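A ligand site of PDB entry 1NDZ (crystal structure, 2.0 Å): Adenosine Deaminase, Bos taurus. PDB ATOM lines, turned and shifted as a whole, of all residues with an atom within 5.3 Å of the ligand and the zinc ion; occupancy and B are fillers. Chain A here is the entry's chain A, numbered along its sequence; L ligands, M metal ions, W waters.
Within 4 Å of the zinc ion: His 14, His 16, His 213 and Asp 294. The nearest printed residue that does not touch the zinc ion is His 237 (4.02 Å).
ND1 of His 16 is in hydrogen-bond range of O2 of the ligand (3.0 Å). OD1 of Asp 295 is in hydrogen-bond range of N2 of the ligand. OD2 of Asp 18 lies within hydrogen-bond range of O2 of the ligand (2.7 Å).
The zinc ion is bound by NE2 of His 16, 1.9 Å away. The zinc ion is bound by water W6 (1.9 Å). NE2 of His 14 binds the zinc ion (2.0 Å). NE2 of His 213 binds the zinc ion (2.2 Å). The zinc ion is bound by OD2 of Asp 294.
The backbone NH of Cys 152 lies within hydrogen-bond range of the backbone carbonyl oxygen of Tyr 101 (3.0 Å). The side-chain hydroxyl (OG) of Ser 102 lies within hydrogen-bond range of the backbone NH (N) of Leu 105 (3.3 Å). The backbone carbonyl oxygen of Leu 105 lies within hydrogen-bond range of the indole nitrogen of Trp 116, at 2.8 Å. NE2 of His 237 sits at hydrogen-bond distance from OE2 of Glu 216 (3.3 Å). The side-chain carboxylate (OE2) of Glu 185 sits at hydrogen-bond distance from the backbone NH (N) of Glu 216, at 2.9 Å. The backbone NH (N) of Val 217 sits at hydrogen-bond distance from the side-chain carboxylate (OE2) of Glu 185.
Water W6 lies within hydrogen-bond range of the side-chain carboxylate of Asp 294 (2.7 Å) and a ring nitrogen (NE2) of His 237 (2.7 Å). Water W8 bridges an oxygen (O3) of the ligand and the side-chain carboxylate (OD2) of Asp 184. Water W5 lies within hydrogen-bond range of an oxygen (O1) of the ligand (2.7 Å) and the backbone NH (N) of Gly 183 (2.9 Å). Water W3 lies within hydrogen-bond range of OE1 of Glu 216 and O1 of the ligand. Water W2 bridges OE2 of Glu 216 (2.8 Å) and N6 of the ligand (3.1 Å). Water W10 bridges SD of Met 154 (2.9 Å) and SG of Cys 152 (3.2 Å).
O3 of the ligand lies close to O of Gly 183 (3.5 Å). Residues that only touch the ligand: Met 51 (3.9 Å), Leu 55 (3.6 Å), Leu 57 (3.4 Å), Phe 60 (3.0 Å), Leu 61 (3.4 Å), Phe 64 (3.4 Å), Tyr 101 (3.5 Å), Ser 102 (3.7 Å), Leu 105 (3.8 Å), Met 154 (3.5 Å), His 156 (3.98 Å), Asp 184 (3.3 Å), Glu 216 (3.8 Å), Val 217 (3.8 Å) and Thr 268 (3.6 Å). Hydrophobic or aromatic side chains within 4 Å of the ligand: His 16, Met 51, Leu 57, Phe 60, Leu 61, Phe 64, Leu 105, Met 154, His 156 and Val 217. Within 4 Å of the ligand: His 16, Asp 18, Met 51, Leu 55, Leu 57, Phe 60, Leu 61, Phe 64, Tyr 101, Ser 102, Leu 105, Met 154, His 156, Gly 183, Asp 184, Glu 216, Val 217, Thr 268, Asp 294 and Asp 295. Along chain A the residues within 4 Å of the ligand span positions 16 to 295. The nearest printed residue that does not touch the ligand is Leu 267 (4.1 Å).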
ATOM      1  N   HIS A  14      -0.862   3.065 -20.688  1.00  0.00           N
ATOM      2  CA  HIS A  14      -0.075   2.274 -19.648  1.00  0.00           C
ATOM      3  C   HIS A  14      -0.873   2.195 -18.229  1.00  0.00           C
ATOM      4  O   HIS A  14      -0.652   2.932 -17.323  1.00  0.00           O
ATOM      5  CB  HIS A  14       1.416   2.748 -19.510  1.00  0.00           C
ATOM      6  CG  HIS A  14       2.299   1.764 -18.742  1.00  0.00           C
ATOM      7  ND1 HIS A  14       3.507   1.321 -19.169  1.00  0.00           N
ATOM      8  CD2 HIS A  14       2.093   1.213 -17.445  1.00  0.00           C
ATOM      9  CE1 HIS A  14       4.095   0.496 -18.187  1.00  0.00           C
ATOM     10  NE2 HIS A  14       3.302   0.387 -17.142  1.00  0.00           N
ATOM     11  N   HIS A  16      -2.452  -1.237 -15.785  1.00  0.00           N
ATOM     12  CA  HIS A  16      -2.649  -2.706 -15.708  1.00  0.00           C
ATOM     13  C   HIS A  16      -4.047  -3.216 -15.078  1.00  0.00           C
ATOM     14  O   HIS A  16      -4.364  -2.791 -13.960  1.00  0.00           O
ATOM     15  CB  HIS A  16      -1.568  -3.427 -14.711  1.00  0.00           C
ATOM     16  CG  HIS A  16      -0.098  -3.225 -14.991  1.00  0.00           C
ATOM     17  ND1 HIS A  16       0.569  -4.274 -15.435  1.00  0.00           N
ATOM     18  CD2 HIS A  16       0.741  -2.086 -15.007  1.00  0.00           C
ATOM     19  CE1 HIS A  16       1.852  -3.735 -15.694  1.00  0.00           C
ATOM     20  NE2 HIS A  16       2.083  -2.344 -15.535  1.00  0.00           N
ATOM     21  N   ASP A  18      -4.978  -5.777 -13.624  1.00  0.00           N
ATOM     22  CA  ASP A  18      -4.869  -6.408 -12.305  1.00  0.00           C
ATOM     23  C   ASP A  18      -4.428  -5.491 -11.235  1.00  0.00           C
ATOM     24  O   ASP A  18      -4.441  -5.797 -10.014  1.00  0.00           O
ATOM     25  CB  ASP A  18      -4.133  -7.791 -12.248  1.00  0.00           C
ATOM     26  CG  ASP A  18      -2.650  -7.651 -12.869  1.00  0.00           C
ATOM     27  OD1 ASP A  18      -1.748  -8.487 -12.653  1.00  0.00           O
ATOM     28  OD2 ASP A  18      -2.468  -6.746 -13.689  1.00  0.00           O
ATOM     29  N   GLY A  19      -4.037  -4.354 -11.614  1.00  0.00           N
ATOM     30  CA  GLY A  19      -3.965  -3.406 -10.547  1.00  0.00           C
ATOM     31  C   GLY A  19      -4.981  -2.197 -10.673  1.00  0.00           C
ATOM     32  O   GLY A  19      -4.785  -1.106 -10.165  1.00  0.00           O
ATOM     33  N   MET A  51      -0.904   2.533  -1.224  1.00  0.00           N
ATOM     34  CA  MET A  51       0.262   3.113  -0.577  1.00  0.00           C
ATOM     35  C   MET A  51       0.215   4.661  -0.522  1.00  0.00           C
ATOM     36  O   MET A  51      -0.222   5.360  -1.424  1.00  0.00           O
ATOM     37  CB  MET A  51       1.574   2.704  -1.284  1.00  0.00           C
ATOM     38  CG  MET A  51       1.722   1.191  -1.673  1.00  0.00           C
ATOM     39  SD  MET A  51       2.892   1.039  -3.075  1.00  0.00           S
ATOM     40  CE  MET A  51       4.469   1.549  -2.597  1.00  0.00           C
ATOM     41  N   LEU A  55       7.773   1.620  -0.859  1.00  0.00           N
ATOM     42  CA  LEU A  55       8.162   0.491  -0.055  1.00  0.00           C
ATOM     43  C   LEU A  55       9.069  -0.449  -0.814  1.00  0.00           C
ATOM     44  O   LEU A  55       9.434  -0.279  -1.961  1.00  0.00           O
ATOM     45  CB  LEU A  55       6.883  -0.157   0.668  1.00  0.00           C
ATOM     46  CG  LEU A  55       5.542  -0.180   0.010  1.00  0.00           C
ATOM     47  CD1 LEU A  55       5.487  -1.321  -0.993  1.00  0.00           C
ATOM     48  CD2 LEU A  55       4.372  -0.252   0.971  1.00  0.00           C
ATOM     49  N   THR A  56       9.464  -1.524  -0.144  1.00  0.00           N
ATOM     50  CA  THR A  56      10.217  -2.480  -0.976  1.00  0.00           C
ATOM     51  C   THR A  56       9.395  -3.286  -1.987  1.00  0.00           C
ATOM     52  O   THR A  56       8.203  -3.421  -1.810  1.00  0.00           O
ATOM     53  CB  THR A  56      10.982  -3.463  -0.032  1.00  0.00           C
ATOM     54  OG1 THR A  56      11.886  -4.345  -0.746  1.00  0.00           O
ATOM     55  CG2 THR A  56       9.938  -4.186   0.737  1.00  0.00           C
ATOM     56  N   LEU A  57      10.080  -3.905  -2.974  1.00  0.00           N
ATOM     57  CA  LEU A  57       9.295  -4.961  -3.761  1.00  0.00           C
ATOM     58  C   LEU A  57       8.598  -6.056  -3.101  1.00  0.00           C
ATOM     59  O   LEU A  57       7.482  -6.408  -3.376  1.00  0.00           O
ATOM     60  CB  LEU A  57       9.914  -6.016  -4.605  1.00  0.00           C
ATOM     61  CG  LEU A  57      10.322  -5.740  -5.941  1.00  0.00           C
ATOM     62  CD1 LEU A  57      11.259  -4.584  -5.719  1.00  0.00           C
ATOM     63  CD2 LEU A  57      10.734  -6.992  -6.706  1.00  0.00           C
ATOM     64  N   PHE A  60       5.545  -4.608  -1.814  1.00  0.00           N
ATOM     65  CA  PHE A  60       4.676  -4.524  -3.025  1.00  0.00           C
ATOM     66  C   PHE A  60       3.978  -5.781  -3.542  1.00  0.00           C
ATOM     67  O   PHE A  60       2.749  -5.765  -3.760  1.00  0.00           O
ATOM     68  CB  PHE A  60       5.448  -3.698  -4.151  1.00  0.00           C
ATOM     69  CG  PHE A  60       4.541  -3.521  -5.374  1.00  0.00           C
ATOM     70  CD1 PHE A  60       3.382  -2.663  -5.302  1.00  0.00           C
ATOM     71  CD2 PHE A  60       4.869  -4.125  -6.601  1.00  0.00           C
ATOM     72  CE1 PHE A  60       2.672  -2.368  -6.457  1.00  0.00           C
ATOM     73  CE2 PHE A  60       4.083  -3.866  -7.752  1.00  0.00           C
ATOM     74  CZ  PHE A  60       2.996  -2.980  -7.685  1.00  0.00           C
ATOM     75  N   LEU A  61       4.792  -6.891  -3.838  1.00  0.00           N
ATOM     76  CA  LEU A  61       4.145  -8.099  -4.434  1.00  0.00           C
ATOM     77  C   LEU A  61       3.086  -8.799  -3.584  1.00  0.00           C
ATOM     78  O   LEU A  61       2.198  -9.543  -4.026  1.00  0.00           O
ATOM     79  CB  LEU A  61       5.222  -9.125  -4.962  1.00  0.00           C
ATOM     80  CG  LEU A  61       6.382  -8.533  -5.783  1.00  0.00           C
ATOM     81  CD1 LEU A  61       7.427  -9.490  -6.444  1.00  0.00           C
ATOM     82  CD2 LEU A  61       5.810  -8.049  -7.070  1.00  0.00           C
ATOM     83  N   PHE A  64      -0.435  -8.128  -4.311  1.00  0.00           N
ATOM     84  CA  PHE A  64      -1.127  -9.093  -5.195  1.00  0.00           C
ATOM     85  C   PHE A  64      -1.532 -10.431  -4.518  1.00  0.00           C
ATOM     86  O   PHE A  64      -2.553 -11.076  -4.756  1.00  0.00           O
ATOM     87  CB  PHE A  64      -0.298  -9.325  -6.466  1.00  0.00           C
ATOM     88  CG  PHE A  64      -0.293  -8.040  -7.329  1.00  0.00           C
ATOM     89  CD1 PHE A  64       0.836  -7.205  -7.343  1.00  0.00           C
ATOM     90  CD2 PHE A  64      -1.401  -7.769  -8.182  1.00  0.00           C
ATOM     91  CE1 PHE A  64       0.895  -6.086  -8.245  1.00  0.00           C
ATOM     92  CE2 PHE A  64      -1.305  -6.698  -9.134  1.00  0.00           C
ATOM     93  CZ  PHE A  64      -0.179  -5.902  -9.105  1.00  0.00           C
ATOM     94  N   ARG A 100      -3.553  -3.546 -19.907  1.00  0.00           N
ATOM     95  CA  ARG A 100      -2.647  -4.670 -20.075  1.00  0.00           C
ATOM     96  C   ARG A 100      -2.662  -5.519 -18.790  1.00  0.00           C
ATOM     97  O   ARG A 100      -3.090  -5.033 -17.722  1.00  0.00           O
ATOM     98  CB  ARG A 100      -1.182  -4.169 -20.208  1.00  0.00           C
ATOM     99  CG  ARG A 100      -0.526  -3.513 -18.924  1.00  0.00           C
ATOM    100  CD  ARG A 100       0.898  -2.795 -19.205  1.00  0.00           C
ATOM    101  NE  ARG A 100       0.764  -1.956 -20.426  1.00  0.00           N
ATOM    102  CZ  ARG A 100       1.826  -1.393 -20.955  1.00  0.00           C
ATOM    103  NH1 ARG A 100       2.994  -1.887 -20.605  1.00  0.00           N
ATOM    104  NH2 ARG A 100       1.799  -0.321 -21.834  1.00  0.00           N
ATOM    105  N   TYR A 101      -2.218  -6.755 -19.055  1.00  0.00           N
ATOM    106  CA  TYR A 101      -2.258  -7.806 -18.034  1.00  0.00           C
ATOM    107  C   TYR A 101      -1.627  -9.033 -18.433  1.00  0.00           C
ATOM    108  O   TYR A 101      -1.528  -9.321 -19.606  1.00  0.00           O
ATOM    109  CB  TYR A 101      -3.783  -8.059 -17.476  1.00  0.00           C
ATOM    110  CG  TYR A 101      -4.637  -8.731 -18.616  1.00  0.00           C
ATOM    111  CD1 TYR A 101      -4.826 -10.173 -18.585  1.00  0.00           C
ATOM    112  CD2 TYR A 101      -5.133  -7.945 -19.695  1.00  0.00           C
ATOM    113  CE1 TYR A 101      -5.345 -10.831 -19.662  1.00  0.00           C
ATOM    114  CE2 TYR A 101      -5.696  -8.609 -20.766  1.00  0.00           C
ATOM    115  CZ  TYR A 101      -5.820 -10.003 -20.714  1.00  0.00           C
ATOM    116  OH  TYR A 101      -6.497 -10.620 -21.692  1.00  0.00           O
ATOM    117  N   SER A 102      -1.211  -9.896 -17.484  1.00  0.00           N
ATOM    118  CA  SER A 102      -0.798 -11.190 -17.841  1.00  0.00           C
ATOM    119  C   SER A 102      -1.940 -12.200 -17.732  1.00  0.00           C
ATOM    120  O   SER A 102      -2.451 -12.350 -16.630  1.00  0.00           O
ATOM    121  CB  SER A 102       0.316 -11.546 -16.895  1.00  0.00           C
ATOM    122  OG  SER A 102       0.409 -13.062 -16.805  1.00  0.00           O
ATOM    123  N   LEU A 105      -1.593 -14.881 -14.946  1.00  0.00           N
ATOM    124  CA  LEU A 105      -1.771 -14.490 -13.578  1.00  0.00           C
ATOM    125  C   LEU A 105      -3.300 -14.493 -13.020  1.00  0.00           C
ATOM    126  O   LEU A 105      -3.598 -14.249 -11.845  1.00  0.00           O
ATOM    127  CB  LEU A 105      -0.994 -13.205 -13.255  1.00  0.00           C
ATOM    128  CG  LEU A 105       0.568 -13.377 -13.403  1.00  0.00           C
ATOM    129  CD1 LEU A 105       1.316 -12.048 -13.085  1.00  0.00           C
ATOM    130  CD2 LEU A 105       0.994 -14.459 -12.343  1.00  0.00           C
ATOM    131  N   TRP A 116      -0.151 -17.557  -6.999  1.00  0.00           N
ATOM    132  CA  TRP A 116      -0.912 -17.036  -5.793  1.00  0.00           C
ATOM    133  C   TRP A 116      -1.367 -18.156  -4.783  1.00  0.00           C
ATOM    134  O   TRP A 116      -2.457 -18.088  -4.208  1.00  0.00           O
ATOM    135  CB  TRP A 116      -2.261 -16.230  -6.109  1.00  0.00           C
ATOM    136  CG  TRP A 116      -2.006 -15.265  -7.281  1.00  0.00           C
ATOM    137  CD1 TRP A 116      -2.641 -15.273  -8.470  1.00  0.00           C
ATOM    138  CD2 TRP A 116      -1.059 -14.224  -7.516  1.00  0.00           C
ATOM    139  NE1 TRP A 116      -2.259 -14.372  -9.439  1.00  0.00           N
ATOM    140  CE2 TRP A 116      -1.291 -13.632  -8.844  1.00  0.00           C
ATOM    141  CE3 TRP A 116      -0.095 -13.646  -6.679  1.00  0.00           C
ATOM    142  CZ2 TRP A 116      -0.531 -12.582  -9.276  1.00  0.00           C
ATOM    143  CZ3 TRP A 116       0.657 -12.570  -7.176  1.00  0.00           C
ATOM    144  CH2 TRP A 116       0.398 -11.999  -8.453  1.00  0.00           C
ATOM    145  N   CYS A 152       0.955  -9.341 -21.300  1.00  0.00           N
ATOM    146  CA  CYS A 152       2.282  -9.268 -20.763  1.00  0.00           C
ATOM    147  C   CYS A 152       2.887 -10.609 -20.549  1.00  0.00           C
ATOM    148  O   CYS A 152       2.324 -11.497 -19.933  1.00  0.00           O
ATOM    149  CB  CYS A 152       2.039  -8.772 -19.359  1.00  0.00           C
ATOM    150  SG  CYS A 152       1.335  -7.052 -19.129  1.00  0.00           S
ATOM    151  N   MET A 154       6.125 -12.263 -18.609  1.00  0.00           N
ATOM    152  CA  MET A 154       6.625 -11.791 -17.188  1.00  0.00           C
ATOM    153  C   MET A 154       8.159 -12.143 -17.125  1.00  0.00           C
ATOM    154  O   MET A 154       8.532 -13.251 -17.409  1.00  0.00           O
ATOM    155  CB  MET A 154       5.872 -12.722 -16.061  1.00  0.00           C
ATOM    156  CG  MET A 154       4.288 -12.500 -16.022  1.00  0.00           C
ATOM    157  SD  MET A 154       4.115 -10.728 -15.514  1.00  0.00           S
ATOM    158  CE  MET A 154       4.810 -10.267 -14.077  1.00  0.00           C
ATOM    159  N   HIS A 156      10.394 -13.146 -15.076  1.00  0.00           N
ATOM    160  CA  HIS A 156      10.840 -14.368 -14.357  1.00  0.00           C
ATOM    161  C   HIS A 156      10.405 -15.686 -14.912  1.00  0.00           C
ATOM    162  O   HIS A 156      10.738 -16.801 -14.481  1.00  0.00           O
ATOM    163  CB  HIS A 156      10.441 -14.274 -12.868  1.00  0.00           C
ATOM    164  CG  HIS A 156       8.930 -14.334 -12.682  1.00  0.00           C
ATOM    165  ND1 HIS A 156       8.105 -13.279 -12.836  1.00  0.00           N
ATOM    166  CD2 HIS A 156       8.231 -15.473 -12.189  1.00  0.00           C
ATOM    167  CE1 HIS A 156       6.867 -13.679 -12.363  1.00  0.00           C
ATOM    168  NE2 HIS A 156       6.951 -15.068 -12.000  1.00  0.00           N
ATOM    169  N   ALA A 182       6.714  -7.440 -18.623  1.00  0.00           N
ATOM    170  CA  ALA A 182       6.568  -6.846 -17.305  1.00  0.00           C
ATOM    171  C   ALA A 182       7.110  -7.867 -16.165  1.00  0.00           C
ATOM    172  O   ALA A 182       7.621  -8.933 -16.431  1.00  0.00           O
ATOM    173  CB  ALA A 182       5.072  -6.917 -17.092  1.00  0.00           C
ATOM    174  N   GLY A 183       7.055  -7.399 -14.882  1.00  0.00           N
ATOM    175  CA  GLY A 183       7.872  -8.055 -13.814  1.00  0.00           C
ATOM    176  C   GLY A 183       9.021  -7.357 -13.302  1.00  0.00           C
ATOM    177  O   GLY A 183       9.200  -6.164 -13.434  1.00  0.00           O
ATOM    178  N   ASP A 184       9.889  -8.182 -12.722  1.00  0.00           N
ATOM    179  CA  ASP A 184      11.137  -7.607 -12.216  1.00  0.00           C
ATOM    180  C   ASP A 184      12.280  -7.388 -13.219  1.00  0.00           C
ATOM    181  O   ASP A 184      12.977  -8.318 -13.660  1.00  0.00           O
ATOM    182  CB  ASP A 184      11.533  -8.391 -10.889  1.00  0.00           C
ATOM    183  CG  ASP A 184      12.816  -7.785 -10.329  1.00  0.00           C
ATOM    184  OD1 ASP A 184      13.424  -8.457  -9.511  1.00  0.00           O
ATOM    185  OD2 ASP A 184      13.371  -6.781 -10.737  1.00  0.00           O
ATOM    186  N   GLU A 185      12.368  -6.111 -13.566  1.00  0.00           N
ATOM    187  CA  GLU A 185      13.308  -5.824 -14.696  1.00  0.00           C
ATOM    188  C   GLU A 185      14.762  -5.808 -14.226  1.00  0.00           C
ATOM    189  O   GLU A 185      15.670  -5.669 -15.022  1.00  0.00           O
ATOM    190  CB  GLU A 185      13.034  -4.561 -15.518  1.00  0.00           C
ATOM    191  CG  GLU A 185      13.222  -3.255 -14.809  1.00  0.00           C
ATOM    192  CD  GLU A 185      13.413  -1.949 -15.521  1.00  0.00           C
ATOM    193  OE1 GLU A 185      14.343  -1.792 -16.337  1.00  0.00           O
ATOM    194  OE2 GLU A 185      12.627  -1.083 -15.134  1.00  0.00           O
ATOM    195  N   HIS A 213       8.280  -2.940 -20.540  1.00  0.00           N
ATOM    196  CA  HIS A 213       8.704  -2.177 -19.421  1.00  0.00           C
ATOM    197  C   HIS A 213      10.262  -2.189 -19.195  1.00  0.00           C
ATOM    198  O   HIS A 213      10.900  -3.206 -19.104  1.00  0.00           O
ATOM    199  CB  HIS A 213       8.178  -2.632 -17.932  1.00  0.00           C
ATOM    200  CG  HIS A 213       6.719  -2.565 -17.661  1.00  0.00           C
ATOM    201  ND1 HIS A 213       5.865  -3.114 -18.405  1.00  0.00           N
ATOM    202  CD2 HIS A 213       6.041  -2.027 -16.538  1.00  0.00           C
ATOM    203  CE1 HIS A 213       4.640  -2.964 -17.828  1.00  0.00           C
ATOM    204  NE2 HIS A 213       4.716  -2.325 -16.681  1.00  0.00           N
ATOM    205  N   GLU A 216      12.639   1.726 -15.694  1.00  0.00           N
ATOM    206  CA  GLU A 216      11.799   2.179 -14.544  1.00  0.00           C
ATOM    207  C   GLU A 216      12.631   2.198 -13.229  1.00  0.00           C
ATOM    208  O   GLU A 216      12.845   3.274 -12.675  1.00  0.00           O
ATOM    209  CB  GLU A 216      10.481   1.396 -14.360  1.00  0.00           C
ATOM    210  CG  GLU A 216       9.676   1.789 -13.074  1.00  0.00           C
ATOM    211  CD  GLU A 216       8.497   0.915 -12.863  1.00  0.00           C
ATOM    212  OE1 GLU A 216       8.621  -0.151 -13.335  1.00  0.00           O
ATOM    213  OE2 GLU A 216       7.541   1.190 -12.155  1.00  0.00           O
ATOM    214  N   VAL A 217      13.105   0.985 -12.971  1.00  0.00           N
ATOM    215  CA  VAL A 217      14.010   0.656 -11.858  1.00  0.00           C
ATOM    216  C   VAL A 217      15.345  -0.021 -12.332  1.00  0.00           C
ATOM    217  O   VAL A 217      16.389  -0.016 -11.671  1.00  0.00           O
ATOM    218  CB  VAL A 217      13.168  -0.022 -10.861  1.00  0.00           C
ATOM    219  CG1 VAL A 217      12.874  -1.447 -10.882  1.00  0.00           C
ATOM    220  CG2 VAL A 217      12.652   0.896  -9.723  1.00  0.00           C
ATOM    221  N   HIS A 237       7.754   3.427 -19.048  1.00  0.00           N
ATOM    222  CA  HIS A 237       8.441   4.357 -18.140  1.00  0.00           C
ATOM    223  C   HIS A 237       9.759   4.845 -18.846  1.00  0.00           C
ATOM    224  O   HIS A 237       9.918   5.907 -19.403  1.00  0.00           O
ATOM    225  CB  HIS A 237       8.903   3.657 -16.877  1.00  0.00           C
ATOM    226  CG  HIS A 237       7.790   3.085 -16.018  1.00  0.00           C
ATOM    227  ND1 HIS A 237       7.045   3.874 -15.239  1.00  0.00           N
ATOM    228  CD2 HIS A 237       7.293   1.782 -15.933  1.00  0.00           C
ATOM    229  CE1 HIS A 237       6.044   3.171 -14.671  1.00  0.00           C
ATOM    230  NE2 HIS A 237       6.206   1.838 -15.069  1.00  0.00           N
ATOM    231  N   LEU A 267       5.875   6.558  -5.833  1.00  0.00           N
ATOM    232  CA  LEU A 267       5.620   5.450  -4.948  1.00  0.00           C
ATOM    233  C   LEU A 267       6.370   4.188  -5.166  1.00  0.00           C
ATOM    234  O   LEU A 267       6.287   3.220  -4.389  1.00  0.00           O
ATOM    235  CB  LEU A 267       4.114   4.927  -4.908  1.00  0.00           C
ATOM    236  CG  LEU A 267       3.145   5.831  -4.178  1.00  0.00           C
ATOM    237  CD1 LEU A 267       1.658   5.530  -4.441  1.00  0.00           C
ATOM    238  CD2 LEU A 267       3.610   6.291  -2.796  1.00  0.00           C
ATOM    239  N   THR A 268       7.042   4.118  -6.287  1.00  0.00           N
ATOM    240  CA  THR A 268       7.701   2.842  -6.420  1.00  0.00           C
ATOM    241  C   THR A 268       9.252   2.967  -6.096  1.00  0.00           C
ATOM    242  O   THR A 268      10.003   2.042  -6.325  1.00  0.00           O
ATOM    243  CB  THR A 268       7.542   2.300  -7.811  1.00  0.00           C
ATOM    244  OG1 THR A 268       8.258   3.133  -8.738  1.00  0.00           O
ATOM    245  CG2 THR A 268       6.030   2.092  -8.172  1.00  0.00           C
ATOM    246  N   ASP A 294      -0.840   3.421 -14.342  1.00  0.00           N
ATOM    247  CA  ASP A 294      -0.237   2.112 -14.005  1.00  0.00           C
ATOM    248  C   ASP A 294      -1.054   1.189 -13.146  1.00  0.00           C
ATOM    249  O   ASP A 294      -1.497   0.140 -13.612  1.00  0.00           O
ATOM    250  CB  ASP A 294       1.175   2.420 -13.268  1.00  0.00           C
ATOM    251  CG  ASP A 294       2.254   1.367 -13.531  1.00  0.00           C
ATOM    252  OD1 ASP A 294       3.328   1.565 -12.921  1.00  0.00           O
ATOM    253  OD2 ASP A 294       2.036   0.437 -14.340  1.00  0.00           O
ATOM    254  N   ASP A 295      -1.260   1.617 -11.806  1.00  0.00           N
ATOM    255  CA  ASP A 295      -2.001   0.656 -10.896  1.00  0.00           C
ATOM    256  C   ASP A 295      -2.737   1.630  -9.844  1.00  0.00           C
ATOM    257  O   ASP A 295      -2.320   1.807  -8.711  1.00  0.00           O
ATOM    258  CB  ASP A 295      -1.058  -0.212  -9.995  1.00  0.00           C
ATOM    259  CG  ASP A 295      -0.183  -1.113 -10.845  1.00  0.00           C
ATOM    260  OD1 ASP A 295      -0.489  -2.279 -10.956  1.00  0.00           O
ATOM    261  OD2 ASP A 295       0.685  -0.615 -11.503  1.00  0.00           O
ATOM    262  N   PHE A 299      -1.996   2.652  -6.063  1.00  0.00           N
ATOM    263  CA  PHE A 299      -1.469   3.953  -5.726  1.00  0.00           C
ATOM    264  C   PHE A 299      -2.560   4.919  -5.263  1.00  0.00           C
ATOM    265  O   PHE A 299      -2.390   6.154  -5.310  1.00  0.00           O
ATOM    266  CB  PHE A 299      -0.722   4.477  -6.984  1.00  0.00           C
ATOM    267  CG  PHE A 299       0.277   3.442  -7.595  1.00  0.00           C
ATOM    268  CD1 PHE A 299       1.119   2.690  -6.649  1.00  0.00           C
ATOM    269  CD2 PHE A 299       0.412   3.122  -8.970  1.00  0.00           C
ATOM    270  CE1 PHE A 299       2.218   1.938  -7.060  1.00  0.00           C
ATOM    271  CE2 PHE A 299       1.450   2.285  -9.382  1.00  0.00           C
ATOM    272  CZ  PHE A 299       2.398   1.769  -8.457  1.00  0.00           C
HETATM  273  C1  LIG L   1       2.624  -5.515 -12.840  1.00  0.00           C
HETATM  274  N1  LIG L   1       1.361  -6.065 -12.743  1.00  0.00           N
HETATM  275  C2  LIG L   1       0.553  -5.065 -12.277  1.00  0.00           C
HETATM  276  N2  LIG L   1       1.200  -4.017 -11.991  1.00  0.00           N
HETATM  277  C3  LIG L   1       2.558  -4.334 -12.287  1.00  0.00           C
HETATM  278  C4  LIG L   1       3.698  -3.450 -12.061  1.00  0.00           C
HETATM  279  O1  LIG L   1       4.894  -3.861 -12.102  1.00  0.00           O
HETATM  280  N3  LIG L   1       3.356  -2.223 -11.722  1.00  0.00           N
HETATM  281  C5  LIG L   1       1.028  -7.509 -12.939  1.00  0.00           C
HETATM  282  C6  LIG L   1       0.621  -7.950 -14.420  1.00  0.00           C
HETATM  283  O2  LIG L   1      -0.287  -7.161 -15.200  1.00  0.00           O
HETATM  284  C7  LIG L   1       2.180  -8.436 -12.558  1.00  0.00           C
HETATM  285  C8  LIG L   1       2.634  -8.267 -11.048  1.00  0.00           C
HETATM  286  N4  LIG L   1       3.991  -8.993 -10.765  1.00  0.00           N
HETATM  287  C9  LIG L   1       4.124 -10.327 -10.627  1.00  0.00           C
HETATM  288  C10 LIG L   1       5.386 -10.598 -10.331  1.00  0.00           C
HETATM  289  C11 LIG L   1       6.042  -9.297 -10.255  1.00  0.00           C
HETATM  290  C12 LIG L   1       5.132  -8.333 -10.627  1.00  0.00           C
HETATM  291  C13 LIG L   1       7.337  -8.958 -10.159  1.00  0.00           C
HETATM  292  C14 LIG L   1       7.674  -7.700 -10.260  1.00  0.00           C
HETATM  293  C15 LIG L   1       6.745  -6.752 -10.559  1.00  0.00           C
HETATM  294  C16 LIG L   1       5.449  -7.075 -10.682  1.00  0.00           C
HETATM  295  N5  LIG L   1       6.965  -5.490 -10.618  1.00  0.00           N
HETATM  296  C17 LIG L   1       8.042  -4.877 -10.501  1.00  0.00           C
HETATM  297  O3  LIG L   1       9.076  -5.347 -10.071  1.00  0.00           O
HETATM  298  C18 LIG L   1       8.024  -3.431 -11.018  1.00  0.00           C
HETATM  299  C19 LIG L   1       8.981  -2.417 -10.354  1.00  0.00           C
HETATM  300  C20 LIG L   1       5.976  -0.824  -5.293  1.00  0.00           C
HETATM  301  C21 LIG L   1       5.887  -1.181  -6.650  1.00  0.00           C
HETATM  302  C22 LIG L   1       6.975  -1.586  -7.392  1.00  0.00           C
HETATM  303  C23 LIG L   1       8.291  -1.414  -6.902  1.00  0.00           C
HETATM  304  C24 LIG L   1       8.427  -1.091  -5.572  1.00  0.00           C
HETATM  305  C25 LIG L   1       7.267  -0.730  -4.798  1.00  0.00           C
HETATM  306  N6  LIG L   1       7.101  -1.991  -8.692  1.00  0.00           N
HETATM  307  C26 LIG L   1       8.412  -2.111  -8.962  1.00  0.00           C
HETATM  308  N7  LIG L   1       9.175  -1.844  -7.908  1.00  0.00           N
HETATM  309  C27 LIG L   1      10.625  -1.923  -7.805  1.00  0.00           C
HETATM  310 ZN    ZN M   1       3.369  -0.938 -15.675  1.00  0.00          ZN
HETATM  311  O   HOH W   1       7.899  -5.376  -7.198  1.00  0.00           O
HETATM  312  O   HOH W   2       5.619  -0.342 -10.792  1.00  0.00           O
HETATM  313  O   HOH W   3       6.804  -2.002 -13.341  1.00  0.00           O
HETATM  314  O   HOH W   4       8.998   1.843  -3.409  1.00  0.00           O
HETATM  315  O   HOH W   5       5.687  -4.871 -14.436  1.00  0.00           O
HETATM  316  O   HOH W   6       4.634  -0.226 -14.417  1.00  0.00           O
HETATM  317  O   HOH W   7       7.513 -12.812  -8.667  1.00  0.00           O
HETATM  318  O   HOH W   8      11.538  -5.116  -9.362  1.00  0.00           O
HETATM  319  O   HOH W   9       3.319  -7.791  -8.373  1.00  0.00           O
HETATM  320  O   HOH W  10       2.776  -8.451 -16.658  1.00  0.00           O
